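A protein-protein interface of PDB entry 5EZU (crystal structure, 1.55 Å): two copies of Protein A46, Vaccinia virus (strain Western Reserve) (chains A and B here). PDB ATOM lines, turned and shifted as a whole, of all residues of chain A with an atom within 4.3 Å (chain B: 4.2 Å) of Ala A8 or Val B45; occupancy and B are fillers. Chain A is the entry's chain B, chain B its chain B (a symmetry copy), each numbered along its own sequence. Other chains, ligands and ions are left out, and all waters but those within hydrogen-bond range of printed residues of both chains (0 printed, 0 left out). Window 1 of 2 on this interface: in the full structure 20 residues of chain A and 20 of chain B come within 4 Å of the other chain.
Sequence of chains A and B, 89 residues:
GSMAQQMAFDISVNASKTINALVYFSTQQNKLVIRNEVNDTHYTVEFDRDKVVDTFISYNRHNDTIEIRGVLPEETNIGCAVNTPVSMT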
ATOM      1  N   MET A   7      -0.943 -23.439 -23.270  1.00  0.00           N
ATOM      2  CA  MET A   7       0.406 -23.584 -23.806  1.00  0.00           C
ATOM      3  C   MET A   7       1.293 -22.444 -23.332  1.00  0.00           C
ATOM      4  O   MET A   7       1.072 -21.290 -23.687  1.00  0.00           O
ATOM      5  CB  MET A   7       0.379 -23.608 -25.331  1.00  0.00           C
ATOM      6  CG  MET A   7      -0.602 -24.593 -25.918  1.00  0.00           C
ATOM      7  SD  MET A   7       0.070 -26.253 -25.958  1.00  0.00           S
ATOM      8  CE  MET A   7      -1.221 -27.135 -25.088  1.00  0.00           C
ATOM      9  N   ALA A   8       2.299 -22.763 -22.533  1.00  0.00           N
ATOM     10  CA  ALA A   8       3.176 -21.730 -22.019  1.00  0.00           C
ATOM     11  C   ALA A   8       4.596 -22.261 -21.815  1.00  0.00           C
ATOM     12  O   ALA A   8       4.807 -23.458 -21.745  1.00  0.00           O
ATOM     13  CB  ALA A   8       2.619 -21.176 -20.724  1.00  0.00           C
ATOM     14  N   PHE A   9       5.577 -21.370 -21.762  1.00  0.00           N
ATOM     15  CA  PHE A   9       6.922 -21.770 -21.365  1.00  0.00           C
ATOM     16  C   PHE A   9       7.521 -20.728 -20.449  1.00  0.00           C
ATOM     17  O   PHE A   9       7.066 -19.575 -20.407  1.00  0.00           O
ATOM     18  CB  PHE A   9       7.820 -21.994 -22.577  1.00  0.00           C
ATOM     19  CG  PHE A   9       8.127 -20.747 -23.337  1.00  0.00           C
ATOM     20  CD1 PHE A   9       7.281 -20.321 -24.345  1.00  0.00           C
ATOM     21  CD2 PHE A   9       9.271 -20.016 -23.061  1.00  0.00           C
ATOM     22  CE1 PHE A   9       7.560 -19.179 -25.054  1.00  0.00           C
ATOM     23  CE2 PHE A   9       9.554 -18.865 -23.772  1.00  0.00           C
ATOM     24  CZ  PHE A   9       8.687 -18.452 -24.772  1.00  0.00           C
ATOM     25  N   TYR A  43      17.526 -24.008 -25.301  1.00  0.00           N
ATOM     26  CA  TYR A  43      16.107 -24.317 -25.126  1.00  0.00           C
ATOM     27  C   TYR A  43      15.319 -23.649 -26.229  1.00  0.00           C
ATOM     28  O   TYR A  43      15.242 -22.430 -26.293  1.00  0.00           O
ATOM     29  CB  TYR A  43      15.594 -23.834 -23.774  1.00  0.00           C
ATOM     30  CG  TYR A  43      14.131 -24.153 -23.529  1.00  0.00           C
ATOM     31  CD1 TYR A  43      13.611 -25.399 -23.849  1.00  0.00           C
ATOM     32  CD2 TYR A  43      13.281 -23.221 -22.954  1.00  0.00           C
ATOM     33  CE1 TYR A  43      12.283 -25.701 -23.615  1.00  0.00           C
ATOM     34  CE2 TYR A  43      11.953 -23.516 -22.712  1.00  0.00           C
ATOM     35  CZ  TYR A  43      11.460 -24.758 -23.047  1.00  0.00           C
ATOM     36  OH  TYR A  43      10.138 -25.062 -22.812  1.00  0.00           O
ATOM     37  N   ARG A  69       8.982 -15.466 -19.571  1.00  0.00           N
ATOM     38  CA  ARG A  69       7.767 -16.267 -19.577  1.00  0.00           C
ATOM     39  C   ARG A  69       7.059 -16.001 -20.893  1.00  0.00           C
ATOM     40  O   ARG A  69       7.009 -14.867 -21.346  1.00  0.00           O
ATOM     41  CB  ARG A  69       6.871 -15.920 -18.392  1.00  0.00           C
ATOM     42  CG  ARG A  69       5.445 -16.405 -18.549  1.00  0.00           C
ATOM     43  CD  ARG A  69       4.915 -17.014 -17.270  1.00  0.00           C
ATOM     44  NE  ARG A  69       3.679 -17.753 -17.503  1.00  0.00           N
ATOM     45  CZ  ARG A  69       3.587 -19.075 -17.433  1.00  0.00           C
ATOM     46  NH1 ARG A  69       4.660 -19.796 -17.140  1.00  0.00           N
ATOM     47  NH2 ARG A  69       2.427 -19.678 -17.661  1.00  0.00           N
ATOM     48  N   GLY A  70       6.531 -17.048 -21.511  1.00  0.00           N
ATOM     49  CA  GLY A  70       5.828 -16.904 -22.773  1.00  0.00           C
ATOM     50  C   GLY A  70       4.478 -17.568 -22.680  1.00  0.00           C
ATOM     51  O   GLY A  70       4.355 -18.664 -22.112  1.00  0.00           O
ATOM     52  N   VAL A  71       3.449 -16.913 -23.200  1.00  0.00           N
ATOM     53  CA  VAL A  71       2.117 -17.515 -23.169  1.00  0.00           C
ATOM     54  C   VAL A  71       1.447 -17.341 -24.516  1.00  0.00           C
ATOM     55  O   VAL A  71       1.817 -16.456 -25.281  1.00  0.00           O
ATOM     56  CB  VAL A  71       1.256 -16.912 -22.047  1.00  0.00           C
ATOM     57  CG1 VAL A  71       1.864 -17.206 -20.679  1.00  0.00           C
ATOM     58  CG2 VAL A  71       1.091 -15.413 -22.256  1.00  0.00           C
ATOM     59  N   PHE B   9       9.266 -28.465 -28.639  1.00  0.00           N
ATOM     60  CA  PHE B   9      10.382 -27.891 -27.895  1.00  0.00           C
ATOM     61  C   PHE B   9      11.581 -28.806 -27.976  1.00  0.00           C
ATOM     62  O   PHE B   9      11.456 -30.000 -28.287  1.00  0.00           O
ATOM     63  CB  PHE B   9      10.009 -27.630 -26.439  1.00  0.00           C
ATOM     64  CG  PHE B   9       9.771 -28.873 -25.648  1.00  0.00           C
ATOM     65  CD1 PHE B   9       8.513 -29.447 -25.615  1.00  0.00           C
ATOM     66  CD2 PHE B   9      10.796 -29.451 -24.917  1.00  0.00           C
ATOM     67  CE1 PHE B   9       8.284 -30.585 -24.883  1.00  0.00           C
ATOM     68  CE2 PHE B   9      10.569 -30.597 -24.180  1.00  0.00           C
ATOM     69  CZ  PHE B   9       9.303 -31.161 -24.169  1.00  0.00           C
ATOM     70  N   LEU B  32      -0.650 -29.760 -17.553  1.00  0.00           N
ATOM     71  CA  LEU B  32       0.455 -30.708 -17.569  1.00  0.00           C
ATOM     72  C   LEU B  32       1.773 -29.950 -17.533  1.00  0.00           C
ATOM     73  O   LEU B  32       2.003 -29.107 -18.390  1.00  0.00           O
ATOM     74  CB  LEU B  32       0.389 -31.578 -18.820  1.00  0.00           C
ATOM     75  CG  LEU B  32       1.584 -32.501 -19.010  1.00  0.00           C
ATOM     76  CD1 LEU B  32       1.544 -33.556 -17.921  1.00  0.00           C
ATOM     77  CD2 LEU B  32       1.573 -33.128 -20.395  1.00  0.00           C
ATOM     78  N   VAL B  33       2.650 -30.246 -16.574  1.00  0.00           N
ATOM     79  CA  VAL B  33       3.906 -29.492 -16.477  1.00  0.00           C
ATOM     80  C   VAL B  33       5.113 -30.377 -16.740  1.00  0.00           C
ATOM     81  O   VAL B  33       5.227 -31.457 -16.179  1.00  0.00           O
ATOM     82  CB  VAL B  33       4.053 -28.814 -15.096  1.00  0.00           C
ATOM     83  CG1 VAL B  33       5.367 -28.037 -15.016  1.00  0.00           C
ATOM     84  CG2 VAL B  33       2.870 -27.928 -14.787  1.00  0.00           C
ATOM     85  N   ILE B  34       6.021 -29.911 -17.592  1.00  0.00           N
ATOM     86  CA  ILE B  34       7.300 -30.567 -17.752  1.00  0.00           C
ATOM     87  C   ILE B  34       8.377 -29.546 -17.426  1.00  0.00           C
ATOM     88  O   ILE B  34       8.557 -28.554 -18.153  1.00  0.00           O
ATOM     89  CB  ILE B  34       7.486 -31.148 -19.156  1.00  0.00           C
ATOM     90  CG1 ILE B  34       6.394 -32.170 -19.455  1.00  0.00           C
ATOM     91  CG2 ILE B  34       8.847 -31.808 -19.266  1.00  0.00           C
ATOM     92  CD1 ILE B  34       6.482 -32.758 -20.850  1.00  0.00           C
ATOM     93  N   THR B  44      10.711 -24.634 -18.400  1.00  0.00           N
ATOM     94  CA  THR B  44       9.432 -25.293 -18.166  1.00  0.00           C
ATOM     95  C   THR B  44       8.512 -25.100 -19.357  1.00  0.00           C
ATOM     96  O   THR B  44       8.466 -24.013 -19.943  1.00  0.00           O
ATOM     97  CB  THR B  44       8.775 -24.719 -16.907  1.00  0.00           C
ATOM     98  OG1 THR B  44       9.677 -24.863 -15.806  1.00  0.00           O
ATOM     99  CG2 THR B  44       7.461 -25.411 -16.605  1.00  0.00           C
ATOM    100  N   VAL B  45       7.799 -26.156 -19.732  1.00  0.00           N
ATOM    101  CA  VAL B  45       6.755 -26.049 -20.724  1.00  0.00           C
ATOM    102  C   VAL B  45       5.479 -26.573 -20.066  1.00  0.00           C
ATOM    103  O   VAL B  45       5.534 -27.471 -19.210  1.00  0.00           O
ATOM    104  CB  VAL B  45       7.124 -26.803 -22.009  1.00  0.00           C
ATOM    105  CG1 VAL B  45       7.197 -28.305 -21.756  1.00  0.00           C
ATOM    106  CG2 VAL B  45       6.168 -26.457 -23.129  1.00  0.00           C
ATOM    107  N   GLU B  46       4.355 -25.966 -20.417  1.00  0.00           N
ATOM    108  CA  GLU B  46       3.072 -26.316 -19.820  1.00  0.00           C
ATOM    109  C   GLU B  46       2.051 -26.521 -20.921  1.00  0.00           C
ATOM    110  O   GLU B  46       2.026 -25.785 -21.910  1.00  0.00           O
ATOM    111  CB  GLU B  46       2.597 -25.231 -18.844  1.00  0.00           C
ATOM    112  CG  GLU B  46       3.661 -24.760 -17.862  1.00  0.00           C
ATOM    113  CD  GLU B  46       3.335 -23.410 -17.244  1.00  0.00           C
ATOM    114  OE1 GLU B  46       2.183 -23.224 -16.794  1.00  0.00           O
ATOM    115  OE2 GLU B  46       4.230 -22.535 -17.210  1.00  0.00           O
ATOM    116  N   PHE B  47       1.208 -27.532 -20.722  1.00  0.00           N
ATOM    117  CA  PHE B  47       0.224 -27.973 -21.698  1.00  0.00           C
ATOM    118  C   PHE B  47      -1.137 -28.183 -21.037  1.00  0.00           C
ATOM    119  O   PHE B  47      -1.222 -28.421 -19.832  1.00  0.00           O
ATOM    120  CB  PHE B  47       0.641 -29.289 -22.368  1.00  0.00           C
ATOM    121  CG  PHE B  47       2.008 -29.271 -22.971  1.00  0.00           C
ATOM    122  CD1 PHE B  47       2.207 -28.818 -24.266  1.00  0.00           C
ATOM    123  CD2 PHE B  47       3.090 -29.742 -22.260  1.00  0.00           C
ATOM    124  CE1 PHE B  47       3.475 -28.808 -24.828  1.00  0.00           C
ATOM    125  CE2 PHE B  47       4.356 -29.742 -22.820  1.00  0.00           C
ATOM    126  CZ  PHE B  47       4.547 -29.274 -24.107  1.00  0.00           C
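The backbone carbonyl oxygen (O) of Ala A8 lies within hydrogen-bond range of the backbone NH (N) of Glu B46, at 2.9 Å. The guanidinium group (NH1) of Arg A69 lies within salt-bridge range of the side-chain carboxylate (OE2) of Glu B46 (2.8 Å). The side-chain hydroxyl (OH) of Tyr A43 lies close to the backbone carbonyl oxygen (O) of Thr B44 (3.5 Å).
The backbone NH of Gly A70 sits at hydrogen-bond distance from the backbone carbonyl oxygen of Phe A9 (2.8 Å). N of Leu B32 sits at hydrogen-bond distance from O of Phe B47 (2.7 Å). The backbone NH (N) of Ile B34 is in hydrogen-bond range of the backbone carbonyl oxygen (O) of Val B45 (3.0 Å).
Among the printed residues, merely in contact across the chains: Phe A9 with Thr B44 (3.1 Å), Met A7 with Glu B46 (3.3 Å), Ala A8 with Val B45 (3.4 Å), Tyr A43 with Val B45 (3.6 Å) and Met A7 with Phe B47 (3.7 Å).
Of the printed residues of chain B, Ala A8 touches Val B45 (3.4 Å) and Glu B46 (2.9 Å). Of the printed residues of chain B, Phe A9 touches Thr B44. Of the printed residues of chain B, Tyr A43 touches Thr B44 (3.5 Å) and Val B45 (3.6 Å). Phe B9 touches none of the printed residues of chain A. Val B33 touches none of the printed residues of chain A. Of the printed residues of chain A, Thr B44 touches Phe A9 and Tyr A43. Of the printed residues of chain A, Val B45 touches Ala A8 (3.4 Å) and Tyr A43 (3.6 Å). Printed residues of chain A within 4 Å of Phe B47: Met A7 (3.7 Å). The nearest printed residue of chain A that does not touch Val B45 is Phe A9 (4.3 Å). The nearest printed residue of chain A that does not touch Phe B47 is Ala A8 (5.2 Å).
Of the 7 printed residues of chain A, 5 touch a printed residue of chain B. Hydrophobic or aromatic side chains of chain A that line the printed part of chain B: Met A7, Phe A9 and Tyr A43. Of the 8 printed residues of chain B, 4 touch a printed residue of chain A. Hydrophobic or aromatic side chains of chain B within 4 Å of the printed part of chain A: Val B45 and Phe B47.
Position printed for both chains: 9.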
